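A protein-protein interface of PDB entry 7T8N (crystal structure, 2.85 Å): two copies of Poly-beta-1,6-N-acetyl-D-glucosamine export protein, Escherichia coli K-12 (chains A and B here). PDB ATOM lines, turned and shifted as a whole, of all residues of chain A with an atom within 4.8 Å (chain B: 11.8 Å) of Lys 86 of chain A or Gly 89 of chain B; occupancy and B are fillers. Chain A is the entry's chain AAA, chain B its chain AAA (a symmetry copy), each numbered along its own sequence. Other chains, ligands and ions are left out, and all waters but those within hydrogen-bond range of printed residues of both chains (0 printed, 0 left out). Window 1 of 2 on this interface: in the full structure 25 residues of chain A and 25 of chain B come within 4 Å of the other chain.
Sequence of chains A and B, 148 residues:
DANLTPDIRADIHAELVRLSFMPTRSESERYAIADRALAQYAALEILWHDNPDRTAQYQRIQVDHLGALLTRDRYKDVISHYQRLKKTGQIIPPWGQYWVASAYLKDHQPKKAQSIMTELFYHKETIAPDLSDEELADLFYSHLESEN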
ATOM      1  N   TYR A  82      -6.005 -17.452 -38.496  1.00  0.00           N
ATOM      2  CA  TYR A  82      -5.674 -16.986 -37.127  1.00  0.00           C
ATOM      3  C   TYR A  82      -6.826 -17.308 -36.174  1.00  0.00           C
ATOM      4  O   TYR A  82      -6.613 -18.017 -35.182  1.00  0.00           O
ATOM      5  CB  TYR A  82      -5.405 -15.488 -37.138  1.00  0.00           C
ATOM      6  CG  TYR A  82      -5.153 -14.871 -35.785  1.00  0.00           C
ATOM      7  CD1 TYR A  82      -3.931 -15.025 -35.151  1.00  0.00           C
ATOM      8  CD2 TYR A  82      -6.115 -14.082 -35.169  1.00  0.00           C
ATOM      9  CE1 TYR A  82      -3.683 -14.445 -33.918  1.00  0.00           C
ATOM     10  CE2 TYR A  82      -5.880 -13.483 -33.945  1.00  0.00           C
ATOM     11  CZ  TYR A  82      -4.657 -13.661 -33.317  1.00  0.00           C
ATOM     12  OH  TYR A  82      -4.404 -13.051 -32.112  1.00  0.00           O
ATOM     13  N   GLN A  83      -8.022 -16.824 -36.516  1.00  0.00           N
ATOM     14  CA  GLN A  83      -9.262 -16.959 -35.705  1.00  0.00           C
ATOM     15  C   GLN A  83      -9.591 -18.439 -35.478  1.00  0.00           C
ATOM     16  O   GLN A  83     -10.085 -18.788 -34.412  1.00  0.00           O
ATOM     17  CB  GLN A  83     -10.419 -16.194 -36.368  1.00  0.00           C
ATOM     18  CG  GLN A  83     -10.564 -14.762 -35.847  1.00  0.00           C
ATOM     19  CD  GLN A  83     -10.651 -14.732 -34.333  1.00  0.00           C
ATOM     20  OE1 GLN A  83     -11.268 -15.606 -33.712  1.00  0.00           O
ATOM     21  NE2 GLN A  83     -10.009 -13.749 -33.708  1.00  0.00           N
ATOM     22  N   ARG A  84      -9.316 -19.277 -36.472  1.00  0.00           N
ATOM     23  CA  ARG A  84      -9.524 -20.747 -36.428  1.00  0.00           C
ATOM     24  C   ARG A  84      -8.478 -21.358 -35.477  1.00  0.00           C
ATOM     25  O   ARG A  84      -8.833 -22.262 -34.711  1.00  0.00           O
ATOM     26  CB  ARG A  84      -9.505 -21.213 -37.888  1.00  0.00           C
ATOM     27  CG  ARG A  84      -9.637 -22.701 -38.162  1.00  0.00           C
ATOM     28  CD  ARG A  84      -9.499 -22.897 -39.668  1.00  0.00           C
ATOM     29  NE  ARG A  84     -10.451 -22.082 -40.418  1.00  0.00           N
ATOM     30  CZ  ARG A  84     -10.163 -21.408 -41.524  1.00  0.00           C
ATOM     31  NH1 ARG A  84      -8.939 -21.437 -42.015  1.00  0.00           N
ATOM     32  NH2 ARG A  84     -11.098 -20.702 -42.128  1.00  0.00           N
ATOM     33  N   LEU A  85      -7.240 -20.857 -35.500  1.00  0.00           N
ATOM     34  CA  LEU A  85      -6.150 -21.306 -34.594  1.00  0.00           C
ATOM     35  C   LEU A  85      -6.471 -20.882 -33.168  1.00  0.00           C
ATOM     36  O   LEU A  85      -6.101 -21.620 -32.228  1.00  0.00           O
ATOM     37  CB  LEU A  85      -4.829 -20.672 -35.027  1.00  0.00           C
ATOM     38  CG  LEU A  85      -3.904 -21.567 -35.840  1.00  0.00           C
ATOM     39  CD1 LEU A  85      -4.660 -22.362 -36.896  1.00  0.00           C
ATOM     40  CD2 LEU A  85      -2.808 -20.737 -36.491  1.00  0.00           C
ATOM     41  N   LYS A  86      -7.099 -19.718 -33.026  1.00  0.00           N
ATOM     42  CA  LYS A  86      -7.489 -19.163 -31.708  1.00  0.00           C
ATOM     43  C   LYS A  86      -8.448 -20.162 -31.042  1.00  0.00           C
ATOM     44  O   LYS A  86      -8.229 -20.518 -29.858  1.00  0.00           O
ATOM     45  CB  LYS A  86      -8.094 -17.757 -31.861  1.00  0.00           C
ATOM     46  CG  LYS A  86      -7.146 -16.566 -31.657  1.00  0.00           C
ATOM     47  CD  LYS A  86      -6.105 -16.731 -30.562  1.00  0.00           C
ATOM     48  CE  LYS A  86      -5.677 -15.411 -29.943  1.00  0.00           C
ATOM     49  NZ  LYS A  86      -4.299 -15.457 -29.373  1.00  0.00           N
ATOM     50  N   LYS A  87      -9.436 -20.642 -31.798  1.00  0.00           N
ATOM     51  CA  LYS A  87     -10.539 -21.490 -31.286  1.00  0.00           C
ATOM     52  C   LYS A  87     -10.057 -22.933 -31.085  1.00  0.00           C
ATOM     53  O   LYS A  87     -10.895 -23.787 -30.775  1.00  0.00           O
ATOM     54  CB  LYS A  87     -11.741 -21.417 -32.231  1.00  0.00           C
ATOM     55  CG  LYS A  87     -12.575 -20.156 -32.069  1.00  0.00           C
ATOM     56  CD  LYS A  87     -13.782 -20.085 -32.970  1.00  0.00           C
ATOM     57  CE  LYS A  87     -14.309 -18.666 -33.094  1.00  0.00           C
ATOM     58  NZ  LYS A  87     -15.420 -18.567 -34.074  1.00  0.00           N
ATOM     59  N   THR A  88      -8.775 -23.225 -31.295  1.00  0.00           N
ATOM     60  CA  THR A  88      -8.137 -24.508 -30.898  1.00  0.00           C
ATOM     61  C   THR A  88      -7.322 -24.287 -29.615  1.00  0.00           C
ATOM     62  O   THR A  88      -6.675 -25.246 -29.139  1.00  0.00           O
ATOM     63  CB  THR A  88      -7.285 -25.075 -32.042  1.00  0.00           C
ATOM     64  OG1 THR A  88      -6.217 -24.161 -32.311  1.00  0.00           O
ATOM     65  CG2 THR A  88      -8.097 -25.336 -33.290  1.00  0.00           C
ATOM     66  N   GLY A  89      -7.319 -23.066 -29.082  1.00  0.00           N
ATOM     67  CA  GLY A  89      -6.582 -22.723 -27.848  1.00  0.00           C
ATOM     68  C   GLY A  89      -5.076 -22.896 -28.003  1.00  0.00           C
ATOM     69  O   GLY A  89      -4.364 -22.907 -26.984  1.00  0.00           O
ATOM     70  N   GLN A  90      -4.595 -22.977 -29.246  1.00  0.00           N
ATOM     71  CA  GLN A  90      -3.157 -23.049 -29.604  1.00  0.00           C
ATOM     72  C   GLN A  90      -2.491 -21.682 -29.350  1.00  0.00           C
ATOM     73  O   GLN A  90      -3.154 -20.601 -29.572  1.00  0.00           O
ATOM     74  CB  GLN A  90      -3.034 -23.460 -31.070  1.00  0.00           C
ATOM     75  CG  GLN A  90      -1.594 -23.597 -31.508  1.00  0.00           C
ATOM     76  CD  GLN A  90      -1.442 -24.060 -32.934  1.00  0.00           C
ATOM     77  OE1 GLN A  90      -2.324 -24.675 -33.527  1.00  0.00           O
ATOM     78  NE2 GLN A  90      -0.284 -23.769 -33.498  1.00  0.00           N
ATOM     79  N   ILE A  92      -0.082 -18.872 -30.337  1.00  0.00           N
ATOM     80  CA  ILE A  92       0.616 -18.280 -31.514  1.00  0.00           C
ATOM     81  C   ILE A  92       1.893 -17.607 -31.016  1.00  0.00           C
ATOM     82  O   ILE A  92       1.854 -16.666 -30.226  1.00  0.00           O
ATOM     83  CB  ILE A  92      -0.299 -17.281 -32.254  1.00  0.00           C
ATOM     84  CG1 ILE A  92      -1.740 -17.778 -32.387  1.00  0.00           C
ATOM     85  CG2 ILE A  92       0.291 -16.883 -33.604  1.00  0.00           C
ATOM     86  CD1 ILE A  92      -1.850 -19.132 -32.996  1.00  0.00           C
ATOM     87  N   THR B  55     -25.192 -19.182 -28.714  1.00  0.00           N
ATOM     88  CA  THR B  55     -23.724 -19.264 -28.492  1.00  0.00           C
ATOM     89  C   THR B  55     -23.351 -18.659 -27.134  1.00  0.00           C
ATOM     90  O   THR B  55     -22.413 -19.170 -26.487  1.00  0.00           O
ATOM     91  CB  THR B  55     -22.961 -18.570 -29.631  1.00  0.00           C
ATOM     92  OG1 THR B  55     -21.573 -18.799 -29.397  1.00  0.00           O
ATOM     93  CG2 THR B  55     -23.214 -17.079 -29.736  1.00  0.00           C
ATOM     94  N   TYR B  58     -24.747 -20.751 -24.127  1.00  0.00           N
ATOM     95  CA  TYR B  58     -23.996 -22.032 -24.201  1.00  0.00           C
ATOM     96  C   TYR B  58     -22.737 -21.900 -23.359  1.00  0.00           C
ATOM     97  O   TYR B  58     -22.556 -22.718 -22.451  1.00  0.00           O
ATOM     98  CB  TYR B  58     -23.591 -22.419 -25.621  1.00  0.00           C
ATOM     99  CG  TYR B  58     -22.920 -23.765 -25.726  1.00  0.00           C
ATOM    100  CD1 TYR B  58     -23.652 -24.928 -25.591  1.00  0.00           C
ATOM    101  CD2 TYR B  58     -21.562 -23.888 -25.954  1.00  0.00           C
ATOM    102  CE1 TYR B  58     -23.064 -26.174 -25.691  1.00  0.00           C
ATOM    103  CE2 TYR B  58     -20.956 -25.129 -26.070  1.00  0.00           C
ATOM    104  CZ  TYR B  58     -21.713 -26.281 -25.947  1.00  0.00           C
ATOM    105  OH  TYR B  58     -21.193 -27.546 -26.039  1.00  0.00           O
ATOM    106  N   GLN B  59     -21.940 -20.867 -23.651  1.00  0.00           N
ATOM    107  CA  GLN B  59     -20.615 -20.600 -23.021  1.00  0.00           C
ATOM    108  C   GLN B  59     -20.779 -20.467 -21.497  1.00  0.00           C
ATOM    109  O   GLN B  59     -19.948 -20.993 -20.744  1.00  0.00           O
ATOM    110  CB  GLN B  59     -19.980 -19.349 -23.635  1.00  0.00           C
ATOM    111  CG  GLN B  59     -19.403 -19.536 -25.041  1.00  0.00           C
ATOM    112  CD  GLN B  59     -18.751 -18.260 -25.534  1.00  0.00           C
ATOM    113  OE1 GLN B  59     -19.124 -17.159 -25.124  1.00  0.00           O
ATOM    114  NE2 GLN B  59     -17.767 -18.377 -26.415  1.00  0.00           N
ATOM    115  N   GLN B  62     -21.342 -23.854 -19.896  1.00  0.00           N
ATOM    116  CA  GLN B  62     -20.020 -24.511 -20.049  1.00  0.00           C
ATOM    117  C   GLN B  62     -19.200 -24.237 -18.789  1.00  0.00           C
ATOM    118  O   GLN B  62     -18.656 -25.196 -18.245  1.00  0.00           O
ATOM    119  CB  GLN B  62     -19.284 -24.016 -21.300  1.00  0.00           C
ATOM    120  CG  GLN B  62     -19.870 -24.509 -22.613  1.00  0.00           C
ATOM    121  CD  GLN B  62     -19.830 -26.015 -22.671  1.00  0.00           C
ATOM    122  OE1 GLN B  62     -18.920 -26.621 -23.229  1.00  0.00           O
ATOM    123  NE2 GLN B  62     -20.818 -26.646 -22.064  1.00  0.00           N
ATOM    124  N   VAL B  63     -19.129 -22.984 -18.331  1.00  0.00           N
ATOM    125  CA  VAL B  63     -18.307 -22.646 -17.133  1.00  0.00           C
ATOM    126  C   VAL B  63     -19.075 -23.078 -15.883  1.00  0.00           C
ATOM    127  O   VAL B  63     -18.515 -23.881 -15.115  1.00  0.00           O
ATOM    128  CB  VAL B  63     -17.806 -21.182 -17.097  1.00  0.00           C
ATOM    129  CG1 VAL B  63     -17.127 -20.794 -18.405  1.00  0.00           C
ATOM    130  CG2 VAL B  63     -18.880 -20.163 -16.750  1.00  0.00           C
ATOM    131  N   SER B  80     -10.790 -32.227 -16.817  1.00  0.00           N
ATOM    132  CA  SER B  80     -10.964 -32.693 -18.209  1.00  0.00           C
ATOM    133  C   SER B  80     -11.945 -31.756 -18.925  1.00  0.00           C
ATOM    134  O   SER B  80     -11.680 -31.426 -20.087  1.00  0.00           O
ATOM    135  CB  SER B  80     -11.394 -34.116 -18.234  1.00  0.00           C
ATOM    136  OG  SER B  80     -12.762 -34.200 -17.897  1.00  0.00           O
ATOM    137  N   HIS B  81     -12.997 -31.289 -18.248  1.00  0.00           N
ATOM    138  CA  HIS B  81     -13.935 -30.275 -18.802  1.00  0.00           C
ATOM    139  C   HIS B  81     -13.176 -28.950 -18.985  1.00  0.00           C
ATOM    140  O   HIS B  81     -13.285 -28.345 -20.055  1.00  0.00           O
ATOM    141  CB  HIS B  81     -15.201 -30.132 -17.941  1.00  0.00           C
ATOM    142  CG  HIS B  81     -16.200 -29.167 -18.501  1.00  0.00           C
ATOM    143  ND1 HIS B  81     -16.902 -29.409 -19.680  1.00  0.00           N
ATOM    144  CD2 HIS B  81     -16.607 -27.950 -18.073  1.00  0.00           C
ATOM    145  CE1 HIS B  81     -17.689 -28.376 -19.946  1.00  0.00           C
ATOM    146  NE2 HIS B  81     -17.524 -27.469 -18.969  1.00  0.00           N
ATOM    147  N   TYR B  82     -12.404 -28.525 -17.989  1.00  0.00           N
ATOM    148  CA  TYR B  82     -11.554 -27.313 -18.083  1.00  0.00           C
ATOM    149  C   TYR B  82     -10.680 -27.386 -19.335  1.00  0.00           C
ATOM    150  O   TYR B  82     -10.761 -26.489 -20.185  1.00  0.00           O
ATOM    151  CB  TYR B  82     -10.683 -27.191 -16.841  1.00  0.00           C
ATOM    152  CG  TYR B  82      -9.697 -26.049 -16.858  1.00  0.00           C
ATOM    153  CD1 TYR B  82     -10.113 -24.748 -16.622  1.00  0.00           C
ATOM    154  CD2 TYR B  82      -8.342 -26.278 -17.049  1.00  0.00           C
ATOM    155  CE1 TYR B  82      -9.212 -23.696 -16.615  1.00  0.00           C
ATOM    156  CE2 TYR B  82      -7.426 -25.242 -17.030  1.00  0.00           C
ATOM    157  CZ  TYR B  82      -7.861 -23.945 -16.809  1.00  0.00           C
ATOM    158  OH  TYR B  82      -6.958 -22.911 -16.765  1.00  0.00           O
ATOM    159  N   GLN B  83      -9.903 -28.466 -19.446  1.00  0.00           N
ATOM    160  CA  GLN B  83      -8.929 -28.709 -20.544  1.00  0.00           C
ATOM    161  C   GLN B  83      -9.645 -28.714 -21.899  1.00  0.00           C
ATOM    162  O   GLN B  83      -9.075 -28.256 -22.883  1.00  0.00           O
ATOM    163  CB  GLN B  83      -8.147 -30.007 -20.286  1.00  0.00           C
ATOM    164  CG  GLN B  83      -6.831 -29.773 -19.542  1.00  0.00           C
ATOM    165  CD  GLN B  83      -5.983 -28.723 -20.237  1.00  0.00           C
ATOM    166  OE1 GLN B  83      -5.934 -28.657 -21.470  1.00  0.00           O
ATOM    167  NE2 GLN B  83      -5.328 -27.863 -19.461  1.00  0.00           N
ATOM    168  N   ARG B  84     -10.871 -29.226 -21.931  1.00  0.00           N
ATOM    169  CA  ARG B  84     -11.738 -29.284 -23.136  1.00  0.00           C
ATOM    170  C   ARG B  84     -12.208 -27.855 -23.466  1.00  0.00           C
ATOM    171  O   ARG B  84     -12.243 -27.504 -24.651  1.00  0.00           O
ATOM    172  CB  ARG B  84     -12.818 -30.326 -22.820  1.00  0.00           C
ATOM    173  CG  ARG B  84     -13.901 -30.565 -23.859  1.00  0.00           C
ATOM    174  CD  ARG B  84     -14.883 -31.569 -23.263  1.00  0.00           C
ATOM    175  NE  ARG B  84     -14.219 -32.794 -22.824  1.00  0.00           N
ATOM    176  CZ  ARG B  84     -14.482 -33.431 -21.692  1.00  0.00           C
ATOM    177  NH1 ARG B  84     -15.394 -32.959 -20.864  1.00  0.00           N
ATOM    178  NH2 ARG B  84     -13.826 -34.534 -21.389  1.00  0.00           N
ATOM    179  N   LEU B  85     -12.526 -27.049 -22.450  1.00  0.00           N
ATOM    180  CA  LEU B  85     -12.933 -25.629 -22.618  1.00  0.00           C
ATOM    181  C   LEU B  85     -11.742 -24.816 -23.104  1.00  0.00           C
ATOM    182  O   LEU B  85     -11.951 -23.851 -23.871  1.00  0.00           O
ATOM    183  CB  LEU B  85     -13.415 -25.071 -21.280  1.00  0.00           C
ATOM    184  CG  LEU B  85     -14.926 -25.007 -21.099  1.00  0.00           C
ATOM    185  CD1 LEU B  85     -15.615 -26.268 -21.604  1.00  0.00           C
ATOM    186  CD2 LEU B  85     -15.270 -24.769 -19.636  1.00  0.00           C
ATOM    187  N   LYS B  86     -10.550 -25.180 -22.638  1.00  0.00           N
ATOM    188  CA  LYS B  86      -9.290 -24.498 -23.017  1.00  0.00           C
ATOM    189  C   LYS B  86      -9.124 -24.626 -24.539  1.00  0.00           C
ATOM    190  O   LYS B  86      -8.869 -23.596 -25.212  1.00  0.00           O
ATOM    191  CB  LYS B  86      -8.098 -25.069 -22.230  1.00  0.00           C
ATOM    192  CG  LYS B  86      -7.679 -24.317 -20.959  1.00  0.00           C
ATOM    193  CD  LYS B  86      -7.769 -22.802 -21.028  1.00  0.00           C
ATOM    194  CE  LYS B  86      -6.777 -22.103 -20.114  1.00  0.00           C
ATOM    195  NZ  LYS B  86      -7.233 -20.747 -19.689  1.00  0.00           N
ATOM    196  N   LYS B  87      -9.324 -25.835 -25.065  1.00  0.00           N
ATOM    197  CA  LYS B  87      -9.060 -26.179 -26.483  1.00  0.00           C
ATOM    198  C   LYS B  87     -10.188 -25.653 -27.382  1.00  0.00           C
ATOM    199  O   LYS B  87     -10.171 -25.966 -28.577  1.00  0.00           O
ATOM    200  CB  LYS B  87      -8.871 -27.690 -26.631  1.00  0.00           C
ATOM    201  CG  LYS B  87      -7.495 -28.182 -26.208  1.00  0.00           C
ATOM    202  CD  LYS B  87      -7.282 -29.665 -26.379  1.00  0.00           C
ATOM    203  CE  LYS B  87      -6.107 -30.163 -25.557  1.00  0.00           C
ATOM    204  NZ  LYS B  87      -5.965 -31.639 -25.623  1.00  0.00           N
ATOM    205  N   THR B  88     -11.164 -24.927 -26.841  1.00  0.00           N
ATOM    206  CA  THR B  88     -12.164 -24.158 -27.629  1.00  0.00           C
ATOM    207  C   THR B  88     -11.778 -22.671 -27.615  1.00  0.00           C
ATOM    208  O   THR B  88     -12.521 -21.850 -28.195  1.00  0.00           O
ATOM    209  CB  THR B  88     -13.584 -24.398 -27.098  1.00  0.00           C
ATOM    210  OG1 THR B  88     -13.659 -23.902 -25.758  1.00  0.00           O
ATOM    211  CG2 THR B  88     -13.981 -25.856 -27.155  1.00  0.00           C
ATOM    212  N   GLY B  89     -10.674 -22.321 -26.954  1.00  0.00           N
ATOM    213  CA  GLY B  89     -10.190 -20.927 -26.869  1.00  0.00           C
ATOM    214  C   GLY B  89     -11.174 -20.012 -26.151  1.00  0.00           C
ATOM    215  O   GLY B  89     -11.027 -18.781 -26.243  1.00  0.00           O
ATOM    216  N   GLN B  90     -12.121 -20.594 -25.411  1.00  0.00           N
ATOM    217  CA  GLN B  90     -13.105 -19.877 -24.563  1.00  0.00           C
ATOM    218  C   GLN B  90     -12.393 -19.286 -23.330  1.00  0.00           C
ATOM    219  O   GLN B  90     -11.428 -19.937 -22.781  1.00  0.00           O
ATOM    220  CB  GLN B  90     -14.205 -20.854 -24.151  1.00  0.00           C
ATOM    221  CG  GLN B  90     -15.276 -20.192 -23.314  1.00  0.00           C
ATOM    222  CD  GLN B  90     -16.405 -21.119 -22.944  1.00  0.00           C
ATOM    223  OE1 GLN B  90     -16.669 -22.131 -23.587  1.00  0.00           O
ATOM    224  NE2 GLN B  90     -17.103 -20.756 -21.883  1.00  0.00           N
ATOM    225  N   ILE B  91     -12.809 -18.089 -22.906  1.00  0.00           N
ATOM    226  CA  ILE B  91     -12.141 -17.383 -21.777  1.00  0.00           C
ATOM    227  C   ILE B  91     -12.900 -17.755 -20.506  1.00  0.00           C
ATOM    228  O   ILE B  91     -14.039 -17.316 -20.377  1.00  0.00           O
ATOM    229  CB  ILE B  91     -12.083 -15.855 -22.010  1.00  0.00           C
ATOM    230  CG1 ILE B  91     -11.370 -15.486 -23.323  1.00  0.00           C
ATOM    231  CG2 ILE B  91     -11.463 -15.149 -20.806  1.00  0.00           C
ATOM    232  CD1 ILE B  91     -11.948 -14.260 -24.045  1.00  0.00           C
ATOM    233  N   ILE B  92     -12.252 -18.471 -19.590  1.00  0.00           N
ATOM    234  CA  ILE B  92     -12.821 -18.881 -18.274  1.00  0.00           C
ATOM    235  C   ILE B  92     -12.774 -17.672 -17.342  1.00  0.00           C
ATOM    236  O   ILE B  92     -11.707 -17.152 -17.023  1.00  0.00           O
ATOM    237  CB  ILE B  92     -12.046 -20.080 -17.685  1.00  0.00           C
ATOM    238  CG1 ILE B  92     -11.701 -21.138 -18.734  1.00  0.00           C
ATOM    239  CG2 ILE B  92     -12.781 -20.683 -16.492  1.00  0.00           C
ATOM    240  CD1 ILE B  92     -12.877 -21.613 -19.515  1.00  0.00           C
ATOM    241  N   PRO B  93     -13.917 -17.146 -16.873  1.00  0.00           N
ATOM    242  CA  PRO B  93     -13.874 -16.085 -15.878  1.00  0.00           C
ATOM    243  C   PRO B  93     -13.103 -16.549 -14.646  1.00  0.00           C
ATOM    244  O   PRO B  93     -12.995 -17.747 -14.364  1.00  0.00           O
ATOM    245  CB  PRO B  93     -15.351 -15.836 -15.562  1.00  0.00           C
ATOM    246  CG  PRO B  93     -16.061 -16.291 -16.820  1.00  0.00           C
ATOM    247  CD  PRO B  93     -15.282 -17.505 -17.266  1.00  0.00           C
ATOM    248  N   GLN B  97     -11.897 -20.288 -12.736  1.00  0.00           N
ATOM    249  CA  GLN B  97     -10.509 -20.704 -12.454  1.00  0.00           C
ATOM    250  C   GLN B  97     -10.383 -21.083 -10.979  1.00  0.00           C
ATOM    251  O   GLN B  97      -9.637 -22.034 -10.693  1.00  0.00           O
ATOM    252  CB  GLN B  97      -9.535 -19.640 -12.921  1.00  0.00           C
ATOM    253  CG  GLN B  97      -9.032 -19.929 -14.320  1.00  0.00           C
ATOM    254  CD  GLN B  97      -8.955 -18.629 -15.059  1.00  0.00           C
ATOM    255  OE1 GLN B  97      -7.987 -17.883 -14.940  1.00  0.00           O
ATOM    256  NE2 GLN B  97     -10.018 -18.314 -15.762  1.00  0.00           N
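Printed residues of chain A that touch a printed residue of chain B: Lys 86, Lys 87, Thr 88 and Gly 89. Among the printed residues, 5 pairs touch across the chains.
O of Lys 87 of chain A lies close to O of Lys 87 of chain B (3.2 Å).
Lys 86 of chain A touches Gly 89 of chain B, and with the chains exchanged Gly 89 of chain A touches Lys 86 of chain B. Lys 87 of chain B touches its own counterpart, Lys 87 of chain A. Lys 87 of chain A touches Thr 88 of chain B, and with the chains exchanged Thr 88 of chain A touches Lys 87 of chain B. Positions printed for both chains: 82, 83, 84, 85, 86, 87, 88, 89, 90 and 92. Of the 5 pairs that touch across the chains among the printed residues, 5 have their exchanged pair printed and touching as well.
Among the printed residues, merely in contact across the chains: Lys 87 of chain A with Thr 88 of chain B, Thr 88 of chain A with Lys 87 of chain B, Gly 89 of chain A with Lys 86 of chain B and Lys 86 of chain A with Gly 89 of chain B.
No residue of chain B comes within 4 Å of Tyr 82 of chain A. Arg 84 of chain A touches none of the printed residues of chain B. No residue of chain B comes within 4 Å of Leu 85 of chain A. Printed residues of chain B within 4 Å of Lys 86 of chain A: Gly 89. Lys 87 of chain A touches just these residues of chain B: Lys 87 and Thr 88. Ile 92 of chain A touches none of the printed residues of chain B. Of the printed residues of chain A, Lys 86 of chain B touches Gly 89. Of the printed residues of chain A, Lys 87 of chain B touches Lys 87 and Thr 88. Printed residues of chain A within 4 Å of Thr 88 of chain B: Lys 87 (3.4 Å). Gly 89 of chain B touches just one residue of chain A: Lys 86. The nearest residue of chain B that does not touch Lys 86 of chain A is Thr 88 of chain B (4.7 Å). The nearest residue of chain A that does not touch Gly 89 of chain B is Gly 89 of chain A (4.04 Å).
O of Leu 85 of chain A lies within hydrogen-bond range of OG1 of Thr 88 of chain A, 2.5 Å away. The backbone carbonyl oxygen (O) of Leu 85 of chain B is in hydrogen-bond range of the side-chain hydroxyl (OG1) of Thr 88 of chain B, at 2.5 Å.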
